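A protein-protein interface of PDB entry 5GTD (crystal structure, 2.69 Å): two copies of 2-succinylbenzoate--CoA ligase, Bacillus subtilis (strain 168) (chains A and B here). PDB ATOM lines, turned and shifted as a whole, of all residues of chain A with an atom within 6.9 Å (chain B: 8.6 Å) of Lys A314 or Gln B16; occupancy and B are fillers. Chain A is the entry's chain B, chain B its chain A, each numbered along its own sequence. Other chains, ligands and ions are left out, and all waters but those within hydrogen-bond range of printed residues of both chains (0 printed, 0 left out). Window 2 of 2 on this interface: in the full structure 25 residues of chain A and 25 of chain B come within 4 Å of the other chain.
The guanidinium group (NH2) of Arg B14 lies close to the side-chain hydroxyl (OG1) of Thr B18 (3.3 Å). The backbone carbonyl oxygen of Ile A297 lies within hydrogen-bond range of the backbone NH of Leu A316 (3.0 Å). O of Thr A299 is in hydrogen-bond range of N of Lys A314, 3.0 Å away. The side-chain amino group of Lys A314 is in hydrogen-bond range of the backbone carbonyl oxygen of Glu A376. SG of Cys A319 is in hydrogen-bond range of O of Phe A317, at 3.7 Å.
No position is printed for both chains.
Of the 20 printed residues of chain A, 5 touch a printed residue of chain B. Hydrophobic or aromatic side chains of chain A that line the printed part of chain B: Phe A317. Among the printed residues, 9 pairs touch across the chains.
Lys A314 touches Leu B17. O of Pro A315 touches CD2 of Leu B17 (3.3 Å). CZ of Phe A317 touches O of Trp B10 (3.7 Å). NE2 of Gln B13 touches CA of Phe A317, 3.5 Å away. CD1 of Phe A317 touches NH1 of Arg B14, 3.3 Å away. Phe A317 touches Leu B17 (CD1 to CD1, 3.98 Å).
NE2 of Gln B13 lies within hydrogen-bond range of O of Leu A316 (3.2 Å). The backbone carbonyl oxygen of Cys A319 sits at hydrogen-bond distance from the side-chain amide nitrogen of Gln B13. The side-chain amino group (NZ) of Lys A314 is in hydrogen-bond range of the backbone carbonyl oxygen (O) of Gln B16 (2.7 Å).
No residue of chain B comes within 4 Å of Gly A313. Printed residues of chain B within 4 Å of Lys A314: Gln B16 (2.7 Å) and Leu B17 (3.7 Å). Of the printed residues of chain B, Leu A316 touches Gln B13 (3.2 Å). Of the printed residues of chain B, Phe A317 touches Trp B10, Gln B13, Arg B14 and Leu B17. Printed residues of chain A within 4 Å of Trp B10: Phe A317 (3.7 Å). Of the printed residues of chain A, Gln B13 touches Leu A316 (3.2 Å), Phe A317 (3.5 Å) and Cys A319 (3.1 Å). Of the printed residues of chain A, Arg B14 touches Phe A317 (3.3 Å). The nearest residue of chain A that does not touch Gln B16 is Glu A376 (5.1 Å). The nearest printed residue of chain A that does not touch Arg B14 is Asn A181 (6.4 Å).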
ATOM      1  N   ASN A 181      39.304   0.499  33.050  1.00  0.00           N
ATOM      2  CA  ASN A 181      39.081   0.817  31.647  1.00  0.00           C
ATOM      3  C   ASN A 181      40.311   0.566  30.778  1.00  0.00           C
ATOM      4  O   ASN A 181      40.197   0.045  29.670  1.00  0.00           O
ATOM      5  CB  ASN A 181      38.640   2.274  31.508  1.00  0.00           C
ATOM      6  CG  ASN A 181      38.383   2.671  30.067  1.00  0.00           C
ATOM      7  OD1 ASN A 181      39.146   3.435  29.475  1.00  0.00           O
ATOM      8  ND2 ASN A 181      37.301   2.156  29.495  1.00  0.00           N
ATOM      9  N   ILE A 297      35.481  10.808  32.535  1.00  0.00           N
ATOM     10  CA  ILE A 297      34.346  10.048  33.043  1.00  0.00           C
ATOM     11  C   ILE A 297      33.754   9.228  31.900  1.00  0.00           C
ATOM     12  O   ILE A 297      32.946   8.326  32.110  1.00  0.00           O
ATOM     13  CB  ILE A 297      33.272  10.964  33.674  1.00  0.00           C
ATOM     14  CG1 ILE A 297      32.305  10.140  34.536  1.00  0.00           C
ATOM     15  CG2 ILE A 297      32.545  11.776  32.600  1.00  0.00           C
ATOM     16  CD1 ILE A 297      31.438  10.965  35.457  1.00  0.00           C
ATOM     17  N   VAL A 298      34.184   9.552  30.685  1.00  0.00           N
ATOM     18  CA  VAL A 298      33.790   8.824  29.487  1.00  0.00           C
ATOM     19  C   VAL A 298      34.988   8.695  28.551  1.00  0.00           C
ATOM     20  O   VAL A 298      35.604   9.695  28.195  1.00  0.00           O
ATOM     21  CB  VAL A 298      32.638   9.529  28.743  1.00  0.00           C
ATOM     22  CG1 VAL A 298      32.444   8.918  27.370  1.00  0.00           C
ATOM     23  CG2 VAL A 298      31.348   9.460  29.549  1.00  0.00           C
ATOM     24  N   THR A 299      35.329   7.469  28.165  1.00  0.00           N
ATOM     25  CA  THR A 299      36.431   7.249  27.231  1.00  0.00           C
ATOM     26  C   THR A 299      35.992   6.397  26.042  1.00  0.00           C
ATOM     27  O   THR A 299      34.990   5.684  26.111  1.00  0.00           O
ATOM     28  CB  THR A 299      37.639   6.577  27.917  1.00  0.00           C
ATOM     29  OG1 THR A 299      37.271   5.269  28.374  1.00  0.00           O
ATOM     30  CG2 THR A 299      38.115   7.408  29.097  1.00  0.00           C
ATOM     31  N   LEU A 300      36.752   6.475  24.954  1.00  0.00           N
ATOM     32  CA  LEU A 300      36.392   5.796  23.714  1.00  0.00           C
ATOM     33  C   LEU A 300      37.527   4.899  23.222  1.00  0.00           C
ATOM     34  O   LEU A 300      38.597   5.383  22.853  1.00  0.00           O
ATOM     35  CB  LEU A 300      36.018   6.826  22.642  1.00  0.00           C
ATOM     36  CG  LEU A 300      35.386   6.364  21.325  1.00  0.00           C
ATOM     37  CD1 LEU A 300      36.442   6.094  20.262  1.00  0.00           C
ATOM     38  CD2 LEU A 300      34.507   5.139  21.543  1.00  0.00           C
ATOM     39  N   SER A 301      37.282   3.591  23.218  1.00  0.00           N
ATOM     40  CA  SER A 301      38.277   2.620  22.774  1.00  0.00           C
ATOM     41  C   SER A 301      38.548   2.750  21.278  1.00  0.00           C
ATOM     42  O   SER A 301      37.615   2.899  20.489  1.00  0.00           O
ATOM     43  CB  SER A 301      37.820   1.197  23.104  1.00  0.00           C
ATOM     44  N   SER A 311      32.829  10.141  18.568  1.00  0.00           N
ATOM     45  CA  SER A 311      32.096   9.947  19.813  1.00  0.00           C
ATOM     46  C   SER A 311      32.985  10.147  21.035  1.00  0.00           C
ATOM     47  O   SER A 311      34.203   9.994  20.961  1.00  0.00           O
ATOM     48  CB  SER A 311      31.472   8.552  19.855  1.00  0.00           C
ATOM     49  OG  SER A 311      30.929   8.271  21.134  1.00  0.00           O
ATOM     50  N   ALA A 312      32.363  10.490  22.158  1.00  0.00           N
ATOM     51  CA  ALA A 312      33.081  10.635  23.417  1.00  0.00           C
ATOM     52  C   ALA A 312      33.372   9.264  24.014  1.00  0.00           C
ATOM     53  O   ALA A 312      34.356   9.081  24.732  1.00  0.00           O
ATOM     54  CB  ALA A 312      32.283  11.487  24.391  1.00  0.00           C
ATOM     55  N   GLY A 313      32.507   8.302  23.708  1.00  0.00           N
ATOM     56  CA  GLY A 313      32.674   6.943  24.186  1.00  0.00           C
ATOM     57  C   GLY A 313      31.576   6.514  25.139  1.00  0.00           C
ATOM     58  O   GLY A 313      30.420   6.914  24.995  1.00  0.00           O
ATOM     59  N   LYS A 314      31.944   5.698  26.120  1.00  0.00           N
ATOM     60  CA  LYS A 314      30.996   5.193  27.104  1.00  0.00           C
ATOM     61  C   LYS A 314      31.502   5.510  28.513  1.00  0.00           C
ATOM     62  O   LYS A 314      32.695   5.758  28.695  1.00  0.00           O
ATOM     63  CB  LYS A 314      30.786   3.686  26.914  1.00  0.00           C
ATOM     64  CG  LYS A 314      30.544   3.278  25.468  1.00  0.00           C
ATOM     65  CD  LYS A 314      29.868   1.922  25.365  1.00  0.00           C
ATOM     66  CE  LYS A 314      28.364   2.043  25.550  1.00  0.00           C
ATOM     67  NZ  LYS A 314      27.661   0.779  25.195  1.00  0.00           N
ATOM     68  N   PRO A 315      30.600   5.517  29.511  1.00  0.00           N
ATOM     69  CA  PRO A 315      31.028   5.835  30.880  1.00  0.00           C
ATOM     70  C   PRO A 315      32.057   4.850  31.418  1.00  0.00           C
ATOM     71  O   PRO A 315      32.000   3.662  31.091  1.00  0.00           O
ATOM     72  CB  PRO A 315      29.731   5.736  31.693  1.00  0.00           C
ATOM     73  CG  PRO A 315      28.640   5.866  30.707  1.00  0.00           C
ATOM     74  CD  PRO A 315      29.150   5.271  29.435  1.00  0.00           C
ATOM     75  N   LEU A 316      32.990   5.339  32.227  1.00  0.00           N
ATOM     76  CA  LEU A 316      33.886   4.453  32.951  1.00  0.00           C
ATOM     77  C   LEU A 316      33.072   3.644  33.948  1.00  0.00           C
ATOM     78  O   LEU A 316      31.961   4.038  34.310  1.00  0.00           O
ATOM     79  CB  LEU A 316      34.982   5.237  33.673  1.00  0.00           C
ATOM     80  CG  LEU A 316      35.991   5.982  32.801  1.00  0.00           C
ATOM     81  CD1 LEU A 316      37.204   6.380  33.630  1.00  0.00           C
ATOM     82  CD2 LEU A 316      36.394   5.133  31.608  1.00  0.00           C
ATOM     83  N   PHE A 317      33.616   2.514  34.388  1.00  0.00           N
ATOM     84  CA  PHE A 317      32.927   1.694  35.374  1.00  0.00           C
ATOM     85  C   PHE A 317      32.656   2.523  36.629  1.00  0.00           C
ATOM     86  O   PHE A 317      33.452   3.396  36.982  1.00  0.00           O
ATOM     87  CB  PHE A 317      33.740   0.445  35.709  1.00  0.00           C
ATOM     88  CG  PHE A 317      32.894  -0.735  36.091  1.00  0.00           C
ATOM     89  CD1 PHE A 317      32.364  -1.565  35.115  1.00  0.00           C
ATOM     90  CD2 PHE A 317      32.622  -1.012  37.421  1.00  0.00           C
ATOM     91  CE1 PHE A 317      31.577  -2.652  35.460  1.00  0.00           C
ATOM     92  CE2 PHE A 317      31.836  -2.097  37.772  1.00  0.00           C
ATOM     93  CZ  PHE A 317      31.314  -2.918  36.791  1.00  0.00           C
ATOM     94  N   CYS A 319      30.495   4.708  36.771  1.00  0.00           N
ATOM     95  CA  CYS A 319      30.054   6.035  36.343  1.00  0.00           C
ATOM     96  C   CYS A 319      28.859   5.984  35.394  1.00  0.00           C
ATOM     97  O   CYS A 319      28.655   4.998  34.687  1.00  0.00           O
ATOM     98  CB  CYS A 319      31.211   6.788  35.686  1.00  0.00           C
ATOM     99  SG  CYS A 319      32.669   6.974  36.743  1.00  0.00           S
ATOM    100  N   ILE A 321      26.073   8.383  32.696  1.00  0.00           N
ATOM    101  CA  ILE A 321      25.707   9.596  31.970  1.00  0.00           C
ATOM    102  C   ILE A 321      24.288   9.501  31.418  1.00  0.00           C
ATOM    103  O   ILE A 321      23.826   8.424  31.037  1.00  0.00           O
ATOM    104  CB  ILE A 321      26.674   9.893  30.804  1.00  0.00           C
ATOM    105  CG1 ILE A 321      26.738   8.707  29.839  1.00  0.00           C
ATOM    106  CG2 ILE A 321      28.061  10.231  31.326  1.00  0.00           C
ATOM    107  CD1 ILE A 321      27.625   8.946  28.637  1.00  0.00           C
ATOM    108  N   ASP A 374      23.826   7.478  20.877  1.00  0.00           N
ATOM    109  CA  ASP A 374      23.391   6.683  19.738  1.00  0.00           C
ATOM    110  C   ASP A 374      22.630   5.457  20.225  1.00  0.00           C
ATOM    111  O   ASP A 374      22.393   5.300  21.423  1.00  0.00           O
ATOM    112  CB  ASP A 374      24.579   6.273  18.859  1.00  0.00           C
ATOM    113  CG  ASP A 374      25.645   5.501  19.622  1.00  0.00           C
ATOM    114  OD1 ASP A 374      25.434   5.180  20.811  1.00  0.00           O
ATOM    115  OD2 ASP A 374      26.701   5.210  19.021  1.00  0.00           O
ATOM    116  N   GLU A 376      23.692   2.518  20.417  1.00  0.00           N
ATOM    117  CA  GLU A 376      24.573   1.661  21.202  1.00  0.00           C
ATOM    118  C   GLU A 376      25.050   2.355  22.483  1.00  0.00           C
ATOM    119  O   GLU A 376      25.901   1.834  23.206  1.00  0.00           O
ATOM    120  CB  GLU A 376      25.763   1.212  20.353  1.00  0.00           C
ATOM    121  CG  GLU A 376      25.362   0.398  19.135  1.00  0.00           C
ATOM    122  CD  GLU A 376      26.536  -0.325  18.513  1.00  0.00           C
ATOM    123  OE1 GLU A 376      27.616  -0.337  19.137  1.00  0.00           O
ATOM    124  OE2 GLU A 376      26.386  -0.874  17.403  1.00  0.00           O
ATOM    125  N   GLY A 377      24.481   3.524  22.766  1.00  0.00           N
ATOM    126  CA  GLY A 377      24.727   4.214  24.020  1.00  0.00           C
ATOM    127  C   GLY A 377      25.996   5.043  24.074  1.00  0.00           C
ATOM    128  O   GLY A 377      26.372   5.531  25.140  1.00  0.00           O
ATOM    129  N   PHE A 378      26.661   5.204  22.933  1.00  0.00           N
ATOM    130  CA  PHE A 378      27.863   6.029  22.865  1.00  0.00           C
ATOM    131  C   PHE A 378      27.509   7.507  22.954  1.00  0.00           C
ATOM    132  O   PHE A 378      26.533   7.958  22.355  1.00  0.00           O
ATOM    133  CB  PHE A 378      28.637   5.757  21.576  1.00  0.00           C
ATOM    134  CG  PHE A 378      29.278   4.400  21.527  1.00  0.00           C
ATOM    135  CD1 PHE A 378      28.547   3.283  21.159  1.00  0.00           C
ATOM    136  CD2 PHE A 378      30.615   4.243  21.845  1.00  0.00           C
ATOM    137  CE1 PHE A 378      29.140   2.037  21.111  1.00  0.00           C
ATOM    138  CE2 PHE A 378      31.214   2.998  21.799  1.00  0.00           C
ATOM    139  CZ  PHE A 378      30.475   1.895  21.431  1.00  0.00           C
ATOM    140  N   LEU A 379      28.307   8.259  23.703  1.00  0.00           N
ATOM    141  CA  LEU A 379      28.069   9.686  23.868  1.00  0.00           C
ATOM    142  C   LEU A 379      28.641  10.495  22.713  1.00  0.00           C
ATOM    143  O   LEU A 379      29.809  10.350  22.351  1.00  0.00           O
ATOM    144  CB  LEU A 379      28.663  10.183  25.188  1.00  0.00           C
ATOM    145  CG  LEU A 379      28.579  11.696  25.416  1.00  0.00           C
ATOM    146  CD1 LEU A 379      27.131  12.167  25.424  1.00  0.00           C
ATOM    147  CD2 LEU A 379      29.288  12.097  26.701  1.00  0.00           C
ATOM    148  N   PRO B   8      26.084   1.431  40.087  1.00  0.00           N
ATOM    149  CA  PRO B   8      25.246   0.651  39.172  1.00  0.00           C
ATOM    150  C   PRO B   8      25.541  -0.835  39.323  1.00  0.00           C
ATOM    151  O   PRO B   8      26.688  -1.186  39.604  1.00  0.00           O
ATOM    152  CB  PRO B   8      25.662   1.156  37.788  1.00  0.00           C
ATOM    153  CG  PRO B   8      26.210   2.513  38.032  1.00  0.00           C
ATOM    154  CD  PRO B   8      26.861   2.464  39.382  1.00  0.00           C
ATOM    155  N   ASN B   9      24.525  -1.678  39.169  1.00  0.00           N
ATOM    156  CA  ASN B   9      24.718  -3.121  39.210  1.00  0.00           C
ATOM    157  C   ASN B   9      25.876  -3.513  38.304  1.00  0.00           C
ATOM    158  O   ASN B   9      25.929  -3.108  37.142  1.00  0.00           O
ATOM    159  CB  ASN B   9      23.440  -3.852  38.795  1.00  0.00           C
ATOM    160  CG  ASN B   9      23.569  -5.359  38.901  1.00  0.00           C
ATOM    161  OD1 ASN B   9      24.180  -6.001  38.047  1.00  0.00           O
ATOM    162  ND2 ASN B   9      22.989  -5.931  39.951  1.00  0.00           N
ATOM    163  N   TRP B  10      26.815  -4.275  38.851  1.00  0.00           N
ATOM    164  CA  TRP B  10      28.047  -4.606  38.143  1.00  0.00           C
ATOM    165  C   TRP B  10      27.780  -5.325  36.826  1.00  0.00           C
ATOM    166  O   TRP B  10      28.335  -4.956  35.792  1.00  0.00           O
ATOM    167  CB  TRP B  10      28.949  -5.459  39.030  1.00  0.00           C
ATOM    168  CG  TRP B  10      29.303  -4.805  40.322  1.00  0.00           C
ATOM    169  CD1 TRP B  10      29.399  -3.466  40.565  1.00  0.00           C
ATOM    170  CD2 TRP B  10      29.592  -5.461  41.563  1.00  0.00           C
ATOM    171  NE1 TRP B  10      29.742  -3.247  41.879  1.00  0.00           N
ATOM    172  CE2 TRP B  10      29.866  -4.456  42.513  1.00  0.00           C
ATOM    173  CE3 TRP B  10      29.650  -6.799  41.961  1.00  0.00           C
ATOM    174  CZ2 TRP B  10      30.192  -4.747  43.834  1.00  0.00           C
ATOM    175  CZ3 TRP B  10      29.974  -7.087  43.273  1.00  0.00           C
ATOM    176  CH2 TRP B  10      30.241  -6.066  44.194  1.00  0.00           C
ATOM    177  N   LEU B  11      26.923  -6.342  36.870  1.00  0.00           N
ATOM    178  CA  LEU B  11      26.592  -7.124  35.683  1.00  0.00           C
ATOM    179  C   LEU B  11      25.832  -6.286  34.656  1.00  0.00           C
ATOM    180  O   LEU B  11      26.104  -6.368  33.458  1.00  0.00           O
ATOM    181  CB  LEU B  11      25.774  -8.361  36.068  1.00  0.00           C
ATOM    182  CG  LEU B  11      25.217  -9.230  34.937  1.00  0.00           C
ATOM    183  CD1 LEU B  11      26.301  -9.601  33.932  1.00  0.00           C
ATOM    184  CD2 LEU B  11      24.567 -10.483  35.508  1.00  0.00           C
ATOM    185  N   MET B  12      24.885  -5.483  35.130  1.00  0.00           N
ATOM    186  CA  MET B  12      24.105  -4.619  34.251  1.00  0.00           C
ATOM    187  C   MET B  12      25.009  -3.655  33.486  1.00  0.00           C
ATOM    188  O   MET B  12      24.926  -3.551  32.265  1.00  0.00           O
ATOM    189  CB  MET B  12      23.063  -3.834  35.050  1.00  0.00           C
ATOM    190  CG  MET B  12      22.149  -2.974  34.192  1.00  0.00           C
ATOM    191  SD  MET B  12      21.195  -1.780  35.148  1.00  0.00           S
ATOM    192  CE  MET B  12      22.510  -0.782  35.845  1.00  0.00           C
ATOM    193  N   GLN B  13      25.879  -2.959  34.210  1.00  0.00           N
ATOM    194  CA  GLN B  13      26.774  -1.989  33.591  1.00  0.00           C
ATOM    195  C   GLN B  13      27.808  -2.667  32.696  1.00  0.00           C
ATOM    196  O   GLN B  13      28.132  -2.159  31.621  1.00  0.00           O
ATOM    197  CB  GLN B  13      27.476  -1.145  34.657  1.00  0.00           C
ATOM    198  CG  GLN B  13      28.471  -0.150  34.088  1.00  0.00           C
ATOM    199  CD  GLN B  13      28.920   0.881  35.102  1.00  0.00           C
ATOM    200  OE1 GLN B  13      28.748   0.702  36.309  1.00  0.00           O
ATOM    201  NE2 GLN B  13      29.497   1.973  34.615  1.00  0.00           N
ATOM    202  N   ARG B  14      28.327  -3.808  33.142  1.00  0.00           N
ATOM    203  CA  ARG B  14      29.302  -4.557  32.355  1.00  0.00           C
ATOM    204  C   ARG B  14      28.679  -5.023  31.041  1.00  0.00           C
ATOM    205  O   ARG B  14      29.324  -4.994  29.991  1.00  0.00           O
ATOM    206  CB  ARG B  14      29.840  -5.748  33.153  1.00  0.00           C
ATOM    207  CG  ARG B  14      30.794  -6.648  32.385  1.00  0.00           C
ATOM    208  CD  ARG B  14      31.896  -5.854  31.704  1.00  0.00           C
ATOM    209  NE  ARG B  14      32.682  -5.060  32.646  1.00  0.00           N
ATOM    210  CZ  ARG B  14      33.587  -4.157  32.283  1.00  0.00           C
ATOM    211  NH1 ARG B  14      34.258  -3.478  33.202  1.00  0.00           N
ATOM    212  NH2 ARG B  14      33.816  -3.930  30.998  1.00  0.00           N
ATOM    213  N   ALA B  15      27.418  -5.441  31.103  1.00  0.00           N
ATOM    214  CA  ALA B  15      26.684  -5.818  29.903  1.00  0.00           C
ATOM    215  C   ALA B  15      26.489  -4.607  28.994  1.00  0.00           C
ATOM    216  O   ALA B  15      26.549  -4.722  27.771  1.00  0.00           O
ATOM    217  CB  ALA B  15      25.341  -6.437  30.270  1.00  0.00           C
ATOM    218  N   GLN B  16      26.264  -3.446  29.604  1.00  0.00           N
ATOM    219  CA  GLN B  16      26.064  -2.204  28.862  1.00  0.00           C
ATOM    220  C   GLN B  16      27.331  -1.744  28.151  1.00  0.00           C
ATOM    221  O   GLN B  16      27.271  -1.197  27.050  1.00  0.00           O
ATOM    222  CB  GLN B  16      25.577  -1.095  29.798  1.00  0.00           C
ATOM    223  CG  GLN B  16      24.139  -1.237  30.261  1.00  0.00           C
ATOM    224  CD  GLN B  16      23.757  -0.202  31.299  1.00  0.00           C
ATOM    225  OE1 GLN B  16      24.618   0.391  31.948  1.00  0.00           O
ATOM    226  NE2 GLN B  16      22.460   0.021  31.460  1.00  0.00           N
ATOM    227  N   LEU B  17      28.477  -1.964  28.788  1.00  0.00           N
ATOM    228  CA  LEU B  17      29.752  -1.471  28.273  1.00  0.00           C
ATOM    229  C   LEU B  17      30.374  -2.413  27.246  1.00  0.00           C
ATOM    230  O   LEU B  17      30.646  -2.014  26.115  1.00  0.00           O
ATOM    231  CB  LEU B  17      30.733  -1.243  29.425  1.00  0.00           C
ATOM    232  CG  LEU B  17      30.386  -0.114  30.396  1.00  0.00           C
ATOM    233  CD1 LEU B  17      31.369  -0.083  31.555  1.00  0.00           C
ATOM    234  CD2 LEU B  17      30.362   1.223  29.672  1.00  0.00           C
ATOM    235  N   THR B  18      30.608  -3.658  27.649  1.00  0.00           N
ATOM    236  CA  THR B  18      31.182  -4.660  26.758  1.00  0.00           C
ATOM    237  C   THR B  18      30.268  -5.879  26.679  1.00  0.00           C
ATOM    238  O   THR B  18      30.492  -6.876  27.365  1.00  0.00           O
ATOM    239  CB  THR B  18      32.584  -5.103  27.221  1.00  0.00           C
ATOM    240  OG1 THR B  18      32.502  -5.663  28.537  1.00  0.00           O
ATOM    241  CG2 THR B  18      33.541  -3.921  27.237  1.00  0.00           C
ATOM    242  N   PRO B  19      29.234  -5.797  25.832  1.00  0.00           N
ATOM    243  CA  PRO B  19      28.191  -6.825  25.738  1.00  0.00           C
ATOM    244  C   PRO B  19      28.711  -8.170  25.247  1.00  0.00           C
ATOM    245  O   PRO B  19      28.236  -9.212  25.703  1.00  0.00           O
ATOM    246  CB  PRO B  19      27.203  -6.234  24.721  1.00  0.00           C
ATOM    247  CG  PRO B  19      27.534  -4.776  24.644  1.00  0.00           C
ATOM    248  CD  PRO B  19      29.001  -4.693  24.887  1.00  0.00           C
ATOM    249  N   GLU B  20      29.678  -8.147  24.336  1.00  0.00           N
ATOM    250  CA  GLU B  20      30.097  -9.367  23.654  1.00  0.00           C
ATOM    251  C   GLU B  20      31.408  -9.949  24.175  1.00  0.00           C
ATOM    252  O   GLU B  20      32.015 -10.801  23.526  1.00  0.00           O
ATOM    253  CB  GLU B  20      30.205  -9.109  22.149  1.00  0.00           C
ATOM    254  CG  GLU B  20      28.968  -8.453  21.553  1.00  0.00           C
ATOM    255  CD  GLU B  20      27.677  -9.142  21.966  1.00  0.00           C
ATOM    256  OE1 GLU B  20      27.638 -10.392  21.988  1.00  0.00           O
ATOM    257  OE2 GLU B  20      26.698  -8.429  22.274  1.00  0.00           O
ATOM    258  N   PHE B  33      28.494 -11.422  28.626  1.00  0.00           N
ATOM    259  CA  PHE B  33      27.978 -10.621  29.727  1.00  0.00           C
ATOM    260  C   PHE B  33      26.531 -10.223  29.466  1.00  0.00           C
ATOM    261  O   PHE B  33      25.700 -10.244  30.374  1.00  0.00           O
ATOM    262  CB  PHE B  33      28.848  -9.382  29.949  1.00  0.00           C
ATOM    263  CG  PHE B  33      30.182  -9.688  30.568  1.00  0.00           C
ATOM    264  CD1 PHE B  33      30.274 -10.030  31.907  1.00  0.00           C
ATOM    265  CD2 PHE B  33      31.340  -9.639  29.812  1.00  0.00           C
ATOM    266  CE1 PHE B  33      31.495 -10.318  32.481  1.00  0.00           C
ATOM    267  CE2 PHE B  33      32.567  -9.925  30.380  1.00  0.00           C
ATOM    268  CZ  PHE B  33      32.644 -10.266  31.716  1.00  0.00           C
ATOM    269  N   ALA B  34      26.233  -9.868  28.220  1.00  0.00           N
ATOM    270  CA  ALA B  34      24.865  -9.559  27.828  1.00  0.00           C
ATOM    271  C   ALA B  34      23.966 -10.779  28.031  1.00  0.00           C
ATOM    272  O   ALA B  34      22.836 -10.657  28.508  1.00  0.00           O
ATOM    273  CB  ALA B  34      24.819  -9.090  26.386  1.00  0.00           C
ATOM    274  N   PHE B  37      23.615 -11.411  31.838  1.00  0.00           N
ATOM    275  CA  PHE B  37      22.631 -10.485  32.383  1.00  0.00           C
ATOM    276  C   PHE B  37      21.214 -10.925  32.030  1.00  0.00           C
ATOM    277  O   PHE B  37      20.323 -10.908  32.877  1.00  0.00           O
ATOM    278  CB  PHE B  37      22.881  -9.065  31.872  1.00  0.00           C
ATOM    279  CG  PHE B  37      21.838  -8.075  32.307  1.00  0.00           C
ATOM    280  CD1 PHE B  37      21.833  -7.578  33.598  1.00  0.00           C
ATOM    281  CD2 PHE B  37      20.862  -7.645  31.425  1.00  0.00           C
ATOM    282  CE1 PHE B  37      20.875  -6.672  34.002  1.00  0.00           C
ATOM    283  CE2 PHE B  37      19.901  -6.739  31.825  1.00  0.00           C
ATOM    284  CZ  PHE B  37      19.909  -6.251  33.115  1.00  0.00           C
ATOM    285  N   ILE B 139      14.502  -4.674  37.363  1.00  0.00           N
ATOM    286  CA  ILE B 139      15.520  -5.065  38.333  1.00  0.00           C
ATOM    287  C   ILE B 139      15.958  -3.953  39.283  1.00  0.00           C
ATOM    288  O   ILE B 139      15.567  -2.794  39.137  1.00  0.00           O
ATOM    289  CB  ILE B 139      16.783  -5.573  37.618  1.00  0.00           C
ATOM    290  CG1 ILE B 139      17.428  -4.422  36.838  1.00  0.00           C
ATOM    291  CG2 ILE B 139      16.452  -6.739  36.708  1.00  0.00           C
ATOM    292  CD1 ILE B 139      18.681  -4.799  36.097  1.00  0.00           C
ATOM    293  N   ALA B 141      18.690  -1.699  39.792  1.00  0.00           N
ATOM    294  CA  ALA B 141      19.762  -1.204  38.938  1.00  0.00           C
ATOM    295  C   ALA B 141      20.966  -0.719  39.741  1.00  0.00           C
ATOM    296  O   ALA B 141      22.050  -0.531  39.188  1.00  0.00           O
ATOM    297  CB  ALA B 141      19.243  -0.090  38.044  1.00  0.00           C
